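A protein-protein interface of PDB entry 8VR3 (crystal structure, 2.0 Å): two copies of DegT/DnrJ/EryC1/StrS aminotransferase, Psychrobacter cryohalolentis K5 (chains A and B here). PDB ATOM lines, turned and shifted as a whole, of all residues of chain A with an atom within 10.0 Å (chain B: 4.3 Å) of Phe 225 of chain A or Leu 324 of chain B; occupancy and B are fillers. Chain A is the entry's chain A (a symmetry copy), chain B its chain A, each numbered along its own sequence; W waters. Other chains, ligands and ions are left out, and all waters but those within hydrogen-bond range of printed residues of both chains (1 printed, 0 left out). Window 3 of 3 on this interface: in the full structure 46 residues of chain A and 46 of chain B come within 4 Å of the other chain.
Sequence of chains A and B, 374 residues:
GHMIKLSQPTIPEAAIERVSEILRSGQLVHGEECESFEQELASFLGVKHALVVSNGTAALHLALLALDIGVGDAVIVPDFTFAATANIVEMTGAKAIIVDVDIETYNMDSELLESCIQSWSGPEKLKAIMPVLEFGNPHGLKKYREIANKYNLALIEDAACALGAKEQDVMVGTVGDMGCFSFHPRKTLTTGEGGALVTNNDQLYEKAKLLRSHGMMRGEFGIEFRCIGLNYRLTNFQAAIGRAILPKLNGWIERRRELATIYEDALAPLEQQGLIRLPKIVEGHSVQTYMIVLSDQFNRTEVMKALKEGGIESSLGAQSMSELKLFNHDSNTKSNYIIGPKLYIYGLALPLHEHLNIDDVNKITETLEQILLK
N of His 214 of chain A lies within hydrogen-bond range of O of Leu 230 of chain A (2.8 Å).
The side-chain carboxylate (OE1) of Glu 224 of chain A is in salt-bridge range of the guanidinium group (NH2) of Arg 226 of chain A (2.7 Å).
The backbone carbonyl oxygen of Gly 215 of chain A lies within hydrogen-bond range of the backbone NH of Arg 226 of chain A (2.7 Å).
The guanidinium group of Arg 233 of chain A sits close to a ring nitrogen (NE2) of His 214 of chain A.
N of Ala 83 of chain B is in hydrogen-bond range of OE1 of Gln 319 of chain B (3.1 Å).
The guanidinium group (NH2) of Arg 226 of chain A sits close to the side-chain sulfur (SD) of Met 217 of chain A (3.5 Å).
Among the printed residues, merely in contact across the chains: Phe 225 of chain A with Gln 319 of chain B, His 214 of chain A with Phe 82 of chain B, Arg 226 of chain A with Leu 326 of chain B, Phe 225 of chain A with Ala 83 of chain B, Phe 225 of chain A with Phe 82 of chain B, Phe 225 of chain A with Leu 326 of chain B, Cys 227 of chain A with Leu 326 of chain B, Ile 228 of chain A with Leu 326 of chain B and Phe 225 of chain A with Leu 324 of chain B.
Phe 225 of chain A touches just these residues of chain B: Phe 82, Ala 83, Gln 319, Leu 324 and Leu 326.
Leu 324 of chain B touches one residue of chain A.
No residue of chain A comes within 4 Å of Ser 320 of chain B.
No residue of chain A comes within 4 Å of Met 321 of chain B.
Of the printed residues of chain B, His 214 of chain A touches Phe 82 (3.5 Å).
Of the printed residues of chain B, Arg 226 of chain A touches Leu 326 (3.7 Å).
Of the printed residues of chain B, Cys 227 of chain A touches Leu 326 (3.9 Å).
Of the printed residues of chain A, Phe 82 of chain B touches His 214 (3.5 Å) and Phe 225 (3.7 Å).
The nearest printed residue of chain B that does not touch Phe 225 of chain A is Lys 325 of chain B (6.9 Å).
The nearest residue of chain A that does not touch Leu 324 of chain B is Glu 224 of chain A (6.4 Å).
Hydrophobic or aromatic side chains of chain A within 4 Å of the printed part of chain B: His 214, Phe 225 and Ile 228.
Of the 10 printed residues of chain B, 5 touch a printed residue of chain A.
Printed residues of chain B that touch a printed residue of chain A: Phe 82, Ala 83, Gln 319, Leu 324 and Leu 326.
Hydrophobic or aromatic side chains of chain B within 4 Å of the printed part of chain A: Phe 82, Ala 83, Leu 324 and Leu 326.
Among the printed residues, no Asp or Glu carboxylate lies within 4 Å of a Lys or Arg side-chain nitrogen of the other chain.
No position is printed for both chains.
Of the 9 pairs that touch across the chains among the printed residues, none has its exchanged pair printed and touching as well.
Water W1 bridges O of Leu 324 of chain B (2.6 Å) and O of Phe 225 of chain A (2.8 Å).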
ATOM      1  N   LEU A 210     -19.687  13.629  -4.052  1.00  0.00           N
ATOM      2  CA  LEU A 210     -18.837  12.799  -4.907  1.00  0.00           C
ATOM      3  C   LEU A 210     -19.548  12.402  -6.214  1.00  0.00           C
ATOM      4  O   LEU A 210     -19.002  12.581  -7.290  1.00  0.00           O
ATOM      5  CB  LEU A 210     -18.408  11.552  -4.140  1.00  0.00           C
ATOM      6  CG  LEU A 210     -17.383  11.789  -3.029  1.00  0.00           C
ATOM      7  CD1 LEU A 210     -17.238  10.532  -2.199  1.00  0.00           C
ATOM      8  CD2 LEU A 210     -16.035  12.214  -3.594  1.00  0.00           C
ATOM      9  N   LEU A 211     -20.771  11.905  -6.108  1.00  0.00           N
ATOM     10  CA  LEU A 211     -21.579  11.455  -7.246  1.00  0.00           C
ATOM     11  C   LEU A 211     -21.888  12.580  -8.236  1.00  0.00           C
ATOM     12  O   LEU A 211     -21.885  12.315  -9.438  1.00  0.00           O
ATOM     13  CB  LEU A 211     -22.850  10.797  -6.723  1.00  0.00           C
ATOM     14  CG  LEU A 211     -22.635   9.485  -5.961  1.00  0.00           C
ATOM     15  CD1 LEU A 211     -23.901   9.032  -5.294  1.00  0.00           C
ATOM     16  CD2 LEU A 211     -22.122   8.359  -6.850  1.00  0.00           C
ATOM     17  N   SER A 213     -19.972  14.957  -9.225  1.00  0.00           N
ATOM     18  CA  SER A 213     -18.886  15.374 -10.083  1.00  0.00           C
ATOM     19  C   SER A 213     -17.759  14.341 -10.148  1.00  0.00           C
ATOM     20  O   SER A 213     -16.643  14.609  -9.693  1.00  0.00           O
ATOM     21  CB  SER A 213     -18.391  16.707  -9.607  1.00  0.00           C
ATOM     22  OG  SER A 213     -17.386  17.133 -10.514  1.00  0.00           O
ATOM     23  N   HIS A 214     -18.055  13.143 -10.672  1.00  0.00           N
ATOM     24  CA  HIS A 214     -17.017  12.218 -11.089  1.00  0.00           C
ATOM     25  C   HIS A 214     -16.169  11.711  -9.924  1.00  0.00           C
ATOM     26  O   HIS A 214     -15.027  11.323 -10.111  1.00  0.00           O
ATOM     27  CB  HIS A 214     -16.036  12.901 -12.044  1.00  0.00           C
ATOM     28  CG  HIS A 214     -16.689  13.571 -13.213  1.00  0.00           C
ATOM     29  ND1 HIS A 214     -17.423  12.888 -14.167  1.00  0.00           N
ATOM     30  CD2 HIS A 214     -16.699  14.886 -13.570  1.00  0.00           C
ATOM     31  CE1 HIS A 214     -17.865  13.770 -15.061  1.00  0.00           C
ATOM     32  NE2 HIS A 214     -17.417  14.997 -14.739  1.00  0.00           N
ATOM     33  N   GLY A 215     -16.734  11.671  -8.720  1.00  0.00           N
ATOM     34  CA  GLY A 215     -16.027  11.166  -7.553  1.00  0.00           C
ATOM     35  C   GLY A 215     -14.891  12.076  -7.079  1.00  0.00           C
ATOM     36  O   GLY A 215     -13.967  11.614  -6.428  1.00  0.00           O
ATOM     37  N   MET A 216     -14.961  13.367  -7.387  1.00  0.00           N
ATOM     38  CA  MET A 216     -13.842  14.258  -7.175  1.00  0.00           C
ATOM     39  C   MET A 216     -13.884  14.808  -5.757  1.00  0.00           C
ATOM     40  O   MET A 216     -14.937  15.148  -5.233  1.00  0.00           O
ATOM     41  CB  MET A 216     -13.871  15.416  -8.162  1.00  0.00           C
ATOM     42  CG  MET A 216     -13.396  15.000  -9.527  1.00  0.00           C
ATOM     43  SD  MET A 216     -13.826  16.241 -10.784  1.00  0.00           S
ATOM     44  CE  MET A 216     -12.417  17.312 -10.550  1.00  0.00           C
ATOM     45  N   MET A 217     -12.706  14.943  -5.150  1.00  0.00           N
ATOM     46  CA  MET A 217     -12.615  15.684  -3.901  1.00  0.00           C
ATOM     47  C   MET A 217     -11.224  16.295  -3.764  1.00  0.00           C
ATOM     48  O   MET A 217     -10.278  15.852  -4.420  1.00  0.00           O
ATOM     49  CB  MET A 217     -12.902  14.788  -2.697  1.00  0.00           C
ATOM     50  CG  MET A 217     -11.894  13.709  -2.535  1.00  0.00           C
ATOM     51  SD  MET A 217     -11.497  13.573  -0.802  1.00  0.00           S
ATOM     52  CE  MET A 217     -12.990  12.768  -0.225  1.00  0.00           C
ATOM     53  N   ARG A 218     -11.138  17.331  -2.916  1.00  0.00           N
ATOM     54  CA  ARG A 218      -9.879  18.006  -2.639  1.00  0.00           C
ATOM     55  C   ARG A 218      -9.039  17.130  -1.709  1.00  0.00           C
ATOM     56  O   ARG A 218      -9.463  16.799  -0.606  1.00  0.00           O
ATOM     57  CB  ARG A 218     -10.139  19.388  -2.035  1.00  0.00           C
ATOM     58  CG  ARG A 218     -10.817  20.365  -2.986  1.00  0.00           C
ATOM     59  CD  ARG A 218     -11.438  21.517  -2.214  1.00  0.00           C
ATOM     60  NE  ARG A 218     -12.148  22.498  -3.031  1.00  0.00           N
ATOM     61  CZ  ARG A 218     -12.856  23.521  -2.547  1.00  0.00           C
ATOM     62  NH1 ARG A 218     -13.013  23.672  -1.243  1.00  0.00           N
ATOM     63  NH2 ARG A 218     -13.421  24.393  -3.368  1.00  0.00           N
ATOM     64  N   GLY A 219      -7.867  16.710  -2.197  1.00  0.00           N
ATOM     65  CA  GLY A 219      -6.879  16.023  -1.381  1.00  0.00           C
ATOM     66  C   GLY A 219      -5.630  16.880  -1.141  1.00  0.00           C
ATOM     67  O   GLY A 219      -5.547  18.050  -1.545  1.00  0.00           O
ATOM     68  N   GLU A 220      -4.647  16.245  -0.493  1.00  0.00           N
ATOM     69  CA  GLU A 220      -3.415  16.881  -0.055  1.00  0.00           C
ATOM     70  C   GLU A 220      -2.716  17.577  -1.225  1.00  0.00           C
ATOM     71  O   GLU A 220      -2.272  18.711  -1.093  1.00  0.00           O
ATOM     72  CB  GLU A 220      -2.545  15.804   0.587  1.00  0.00           C
ATOM     73  CG  GLU A 220      -1.259  16.314   1.204  1.00  0.00           C
ATOM     74  CD  GLU A 220      -0.440  15.225   1.874  1.00  0.00           C
ATOM     75  OE1 GLU A 220       0.726  15.495   2.198  1.00  0.00           O
ATOM     76  OE2 GLU A 220      -0.978  14.108   2.077  1.00  0.00           O
ATOM     77  N   PHE A 221      -2.639  16.898  -2.376  1.00  0.00           N
ATOM     78  CA  PHE A 221      -1.968  17.423  -3.555  1.00  0.00           C
ATOM     79  C   PHE A 221      -2.993  17.666  -4.665  1.00  0.00           C
ATOM     80  O   PHE A 221      -2.740  17.342  -5.825  1.00  0.00           O
ATOM     81  CB  PHE A 221      -0.866  16.451  -3.989  1.00  0.00           C
ATOM     82  CG  PHE A 221       0.089  16.072  -2.882  1.00  0.00           C
ATOM     83  CD1 PHE A 221       0.282  14.742  -2.527  1.00  0.00           C
ATOM     84  CD2 PHE A 221       0.787  17.050  -2.178  1.00  0.00           C
ATOM     85  CE1 PHE A 221       1.161  14.400  -1.508  1.00  0.00           C
ATOM     86  CE2 PHE A 221       1.668  16.707  -1.161  1.00  0.00           C
ATOM     87  CZ  PHE A 221       1.851  15.382  -0.827  1.00  0.00           C
ATOM     88  N   GLY A 222      -4.155  18.229  -4.298  1.00  0.00           N
ATOM     89  CA  GLY A 222      -5.184  18.571  -5.265  1.00  0.00           C
ATOM     90  C   GLY A 222      -6.294  17.521  -5.351  1.00  0.00           C
ATOM     91  O   GLY A 222      -6.541  16.760  -4.418  1.00  0.00           O
ATOM     92  N   ILE A 223      -6.964  17.507  -6.505  1.00  0.00           N
ATOM     93  CA  ILE A 223      -8.207  16.782  -6.680  1.00  0.00           C
ATOM     94  C   ILE A 223      -7.882  15.295  -6.742  1.00  0.00           C
ATOM     95  O   ILE A 223      -7.051  14.899  -7.535  1.00  0.00           O
ATOM     96  CB  ILE A 223      -8.944  17.271  -7.944  1.00  0.00           C
ATOM     97  CG1 ILE A 223      -9.826  18.498  -7.677  1.00  0.00           C
ATOM     98  CG2 ILE A 223      -9.767  16.133  -8.536  1.00  0.00           C
ATOM     99  CD1 ILE A 223      -9.169  19.621  -6.911  1.00  0.00           C
ATOM    100  N   GLU A 224      -8.575  14.496  -5.927  1.00  0.00           N
ATOM    101  CA  GLU A 224      -8.498  13.044  -5.975  1.00  0.00           C
ATOM    102  C   GLU A 224      -9.828  12.444  -6.442  1.00  0.00           C
ATOM    103  O   GLU A 224     -10.903  12.967  -6.137  1.00  0.00           O
ATOM    104  CB  GLU A 224      -8.167  12.495  -4.589  1.00  0.00           C
ATOM    105  CG  GLU A 224      -6.884  13.079  -4.018  1.00  0.00           C
ATOM    106  CD  GLU A 224      -6.465  12.567  -2.650  1.00  0.00           C
ATOM    107  OE1 GLU A 224      -7.342  12.361  -1.769  1.00  0.00           O
ATOM    108  OE2 GLU A 224      -5.259  12.432  -2.459  1.00  0.00           O
ATOM    109  N   PHE A 225      -9.727  11.290  -7.106  1.00  0.00           N
ATOM    110  CA  PHE A 225     -10.874  10.596  -7.658  1.00  0.00           C
ATOM    111  C   PHE A 225     -11.225   9.419  -6.757  1.00  0.00           C
ATOM    112  O   PHE A 225     -10.664   8.342  -6.890  1.00  0.00           O
ATOM    113  CB  PHE A 225     -10.572  10.239  -9.119  1.00  0.00           C
ATOM    114  CG  PHE A 225     -10.530  11.445 -10.025  1.00  0.00           C
ATOM    115  CD1 PHE A 225     -11.663  11.870 -10.706  1.00  0.00           C
ATOM    116  CD2 PHE A 225      -9.362  12.174 -10.193  1.00  0.00           C
ATOM    117  CE1 PHE A 225     -11.629  12.995 -11.523  1.00  0.00           C
ATOM    118  CE2 PHE A 225      -9.321  13.288 -11.025  1.00  0.00           C
ATOM    119  CZ  PHE A 225     -10.463  13.709 -11.672  1.00  0.00           C
ATOM    120  N   ARG A 226     -12.159   9.637  -5.836  1.00  0.00           N
ATOM    121  CA  ARG A 226     -12.398   8.676  -4.776  1.00  0.00           C
ATOM    122  C   ARG A 226     -13.362   7.565  -5.168  1.00  0.00           C
ATOM    123  O   ARG A 226     -13.283   6.494  -4.595  1.00  0.00           O
ATOM    124  CB  ARG A 226     -12.942   9.382  -3.534  1.00  0.00           C
ATOM    125  CG  ARG A 226     -11.887  10.264  -2.891  1.00  0.00           C
ATOM    126  CD  ARG A 226     -10.545   9.533  -2.794  1.00  0.00           C
ATOM    127  NE  ARG A 226      -9.612  10.192  -1.893  1.00  0.00           N
ATOM    128  CZ  ARG A 226      -9.886  10.516  -0.633  1.00  0.00           C
ATOM    129  NH1 ARG A 226     -11.003  10.097  -0.056  1.00  0.00           N
ATOM    130  NH2 ARG A 226      -9.029  11.257   0.048  1.00  0.00           N
ATOM    131  N   CYS A 227     -14.315   7.834  -6.067  1.00  0.00           N
ATOM    132  CA  CYS A 227     -15.265   6.818  -6.458  1.00  0.00           C
ATOM    133  C   CYS A 227     -15.763   7.144  -7.847  1.00  0.00           C
ATOM    134  O   CYS A 227     -15.405   8.178  -8.422  1.00  0.00           O
ATOM    135  CB  CYS A 227     -16.430   6.705  -5.479  1.00  0.00           C
ATOM    136  SG  CYS A 227     -17.355   8.245  -5.297  1.00  0.00           S
ATOM    137  N   ILE A 228     -16.567   6.232  -8.376  1.00  0.00           N
ATOM    138  CA  ILE A 228     -17.251   6.449  -9.633  1.00  0.00           C
ATOM    139  C   ILE A 228     -18.373   7.458  -9.402  1.00  0.00           C
ATOM    140  O   ILE A 228     -19.016   7.436  -8.352  1.00  0.00           O
ATOM    141  CB  ILE A 228     -17.745   5.095 -10.161  1.00  0.00           C
ATOM    142  CG1 ILE A 228     -16.555   4.179 -10.479  1.00  0.00           C
ATOM    143  CG2 ILE A 228     -18.649   5.294 -11.361  1.00  0.00           C
ATOM    144  CD1 ILE A 228     -16.876   2.709 -10.419  1.00  0.00           C
ATOM    145  N   GLY A 229     -18.574   8.358 -10.374  1.00  0.00           N
ATOM    146  CA  GLY A 229     -19.672   9.307 -10.301  1.00  0.00           C
ATOM    147  C   GLY A 229     -20.172   9.737 -11.673  1.00  0.00           C
ATOM    148  O   GLY A 229     -19.788   9.157 -12.689  1.00  0.00           O
ATOM    149  N   LEU A 230     -21.015  10.774 -11.640  1.00  0.00           N
ATOM    150  CA  LEU A 230     -21.716  11.353 -12.777  1.00  0.00           C
ATOM    151  C   LEU A 230     -21.248  12.791 -12.950  1.00  0.00           C
ATOM    152  O   LEU A 230     -20.397  13.262 -12.202  1.00  0.00           O
ATOM    153  CB  LEU A 230     -23.219  11.372 -12.450  1.00  0.00           C
ATOM    154  CG  LEU A 230     -23.890  10.012 -12.379  1.00  0.00           C
ATOM    155  CD1 LEU A 230     -25.264  10.142 -11.762  1.00  0.00           C
ATOM    156  CD2 LEU A 230     -24.000   9.420 -13.758  1.00  0.00           C
ATOM    157  N   ARG A 233     -23.295  18.858 -12.297  1.00  0.00           N
ATOM    158  CA  ARG A 233     -22.905  20.174 -11.843  1.00  0.00           C
ATOM    159  C   ARG A 233     -23.809  21.239 -12.466  1.00  0.00           C
ATOM    160  O   ARG A 233     -24.241  21.135 -13.611  1.00  0.00           O
ATOM    161  CB  ARG A 233     -21.450  20.487 -12.229  1.00  0.00           C
ATOM    162  CG  ARG A 233     -20.376  19.628 -11.571  1.00  0.00           C
ATOM    163  CD  ARG A 233     -18.979  20.219 -11.762  1.00  0.00           C
ATOM    164  NE  ARG A 233     -18.543  20.249 -13.173  1.00  0.00           N
ATOM    165  CZ  ARG A 233     -17.930  19.250 -13.817  1.00  0.00           C
ATOM    166  NH1 ARG A 233     -17.791  18.093 -13.192  1.00  0.00           N
ATOM    167  NH2 ARG A 233     -17.456  19.401 -15.057  1.00  0.00           N
ATOM    168  N   PHE B  82     -10.114  11.378 -19.223  1.00  0.00           N
ATOM    169  CA  PHE B  82     -10.736  11.912 -18.028  1.00  0.00           C
ATOM    170  C   PHE B  82     -11.558  10.788 -17.408  1.00  0.00           C
ATOM    171  O   PHE B  82     -12.086   9.951 -18.129  1.00  0.00           O
ATOM    172  CB  PHE B  82     -11.517  13.192 -18.349  1.00  0.00           C
ATOM    173  CG  PHE B  82     -12.145  13.823 -17.137  1.00  0.00           C
ATOM    174  CD1 PHE B  82     -13.526  13.837 -16.974  1.00  0.00           C
ATOM    175  CD2 PHE B  82     -11.356  14.308 -16.101  1.00  0.00           C
ATOM    176  CE1 PHE B  82     -14.098  14.352 -15.821  1.00  0.00           C
ATOM    177  CE2 PHE B  82     -11.931  14.794 -14.940  1.00  0.00           C
ATOM    178  CZ  PHE B  82     -13.306  14.803 -14.800  1.00  0.00           C
ATOM    179  N   ALA B  83     -11.644  10.765 -16.061  1.00  0.00           N
ATOM    180  CA  ALA B  83     -12.317   9.706 -15.328  1.00  0.00           C
ATOM    181  C   ALA B  83     -13.734   9.401 -15.845  1.00  0.00           C
ATOM    182  O   ALA B  83     -14.182   8.263 -15.817  1.00  0.00           O
ATOM    183  CB  ALA B  83     -12.373  10.109 -13.878  1.00  0.00           C
ATOM    184  N   GLN B 319      -5.850  11.589 -16.848  1.00  0.00           N
ATOM    185  CA  GLN B 319      -5.616  10.563 -15.852  1.00  0.00           C
ATOM    186  C   GLN B 319      -5.345   9.208 -16.470  1.00  0.00           C
ATOM    187  O   GLN B 319      -5.689   8.960 -17.606  1.00  0.00           O
ATOM    188  CB  GLN B 319      -6.841  10.386 -14.977  1.00  0.00           C
ATOM    189  CG  GLN B 319      -7.037  11.504 -13.975  1.00  0.00           C
ATOM    190  CD  GLN B 319      -8.139  12.406 -14.435  1.00  0.00           C
ATOM    191  OE1 GLN B 319      -9.305  12.016 -14.482  1.00  0.00           O
ATOM    192  NE2 GLN B 319      -7.752  13.619 -14.795  1.00  0.00           N
ATOM    193  N   SER B 320      -4.732   8.328 -15.664  1.00  0.00           N
ATOM    194  CA  SER B 320      -4.666   6.903 -15.944  1.00  0.00           C
ATOM    195  C   SER B 320      -5.795   6.164 -15.230  1.00  0.00           C
ATOM    196  O   SER B 320      -5.841   6.180 -14.003  1.00  0.00           O
ATOM    197  CB  SER B 320      -3.339   6.325 -15.526  1.00  0.00           C
ATOM    198  OG  SER B 320      -3.378   4.909 -15.589  1.00  0.00           O
ATOM    199  N   MET B 321      -6.669   5.483 -15.985  1.00  0.00           N
ATOM    200  CA  MET B 321      -7.825   4.825 -15.404  1.00  0.00           C
ATOM    201  C   MET B 321      -7.345   3.642 -14.531  1.00  0.00           C
ATOM    202  O   MET B 321      -7.884   3.398 -13.448  1.00  0.00           O
ATOM    203  CB  MET B 321      -8.790   4.301 -16.480  1.00  0.00           C
ATOM    204  CG  MET B 321      -9.427   5.352 -17.353  1.00  0.00           C
ATOM    205  SD  MET B 321     -10.359   6.596 -16.460  1.00  0.00           S
ATOM    206  CE  MET B 321      -9.168   7.908 -16.180  1.00  0.00           C
ATOM    207  N   SER B 322      -6.281   2.954 -14.964  1.00  0.00           N
ATOM    208  CA  SER B 322      -5.739   1.853 -14.179  1.00  0.00           C
ATOM    209  C   SER B 322      -5.176   2.381 -12.857  1.00  0.00           C
ATOM    210  O   SER B 322      -5.473   1.827 -11.804  1.00  0.00           O
ATOM    211  CB  SER B 322      -4.739   1.021 -14.960  1.00  0.00           C
ATOM    212  OG  SER B 322      -3.674   1.829 -15.419  1.00  0.00           O
ATOM    213  N   GLU B 323      -4.475   3.514 -12.896  1.00  0.00           N
ATOM    214  CA  GLU B 323      -3.896   4.066 -11.677  1.00  0.00           C
ATOM    215  C   GLU B 323      -4.988   4.510 -10.695  1.00  0.00           C
ATOM    216  O   GLU B 323      -4.733   4.562  -9.505  1.00  0.00           O
ATOM    217  CB  GLU B 323      -2.941   5.232 -11.971  1.00  0.00           C
ATOM    218  CG  GLU B 323      -1.634   4.818 -12.646  1.00  0.00           C
ATOM    219  CD  GLU B 323      -0.772   3.872 -11.818  1.00  0.00           C
ATOM    220  OE1 GLU B 323      -0.447   2.770 -12.320  1.00  0.00           O
ATOM    221  OE2 GLU B 323      -0.519   4.204 -10.645  1.00  0.00           O
ATOM    222  N   LEU B 324      -6.200   4.862 -11.149  1.00  0.00           N
ATOM    223  CA  LEU B 324      -7.227   5.309 -10.204  1.00  0.00           C
ATOM    224  C   LEU B 324      -7.685   4.180  -9.286  1.00  0.00           C
ATOM    225  O   LEU B 324      -8.217   4.448  -8.206  1.00  0.00           O
ATOM    226  CB  LEU B 324      -8.438   5.905 -10.936  1.00  0.00           C
ATOM    227  CG  LEU B 324      -8.159   7.227 -11.653  1.00  0.00           C
ATOM    228  CD1 LEU B 324      -9.416   7.774 -12.307  1.00  0.00           C
ATOM    229  CD2 LEU B 324      -7.563   8.258 -10.697  1.00  0.00           C
ATOM    230  N   LYS B 325      -7.517   2.929  -9.723  1.00  0.00           N
ATOM    231  CA  LYS B 325      -7.883   1.794  -8.903  1.00  0.00           C
ATOM    232  C   LYS B 325      -9.380   1.775  -8.604  1.00  0.00           C
ATOM    233  O   LYS B 325      -9.781   1.334  -7.544  1.00  0.00           O
ATOM    234  CB  LYS B 325      -7.076   1.787  -7.599  1.00  0.00           C
ATOM    235  CG  LYS B 325      -5.600   1.473  -7.806  1.00  0.00           C
ATOM    236  CD  LYS B 325      -5.422   0.181  -8.584  1.00  0.00           C
ATOM    237  CE  LYS B 325      -4.033  -0.404  -8.429  1.00  0.00           C
ATOM    238  NZ  LYS B 325      -3.032   0.532  -8.982  1.00  0.00           N
ATOM    239  N   LEU B 326     -10.205   2.165  -9.582  1.00  0.00           N
ATOM    240  CA  LEU B 326     -11.650   2.186  -9.414  1.00  0.00           C
ATOM    241  C   LEU B 326     -12.328   1.138 -10.299  1.00  0.00           C
ATOM    242  O   LEU B 326     -13.472   0.780 -10.030  1.00  0.00           O
ATOM    243  CB  LEU B 326     -12.129   3.586  -9.811  1.00  0.00           C
ATOM    244  CG  LEU B 326     -11.751   4.728  -8.882  1.00  0.00           C
ATOM    245  CD1 LEU B 326     -12.307   6.038  -9.424  1.00  0.00           C
ATOM    246  CD2 LEU B 326     -12.276   4.470  -7.474  1.00  0.00           C
HETATM  247  O   HOH W   1      -8.383   6.870  -7.341  1.00  0.00           O
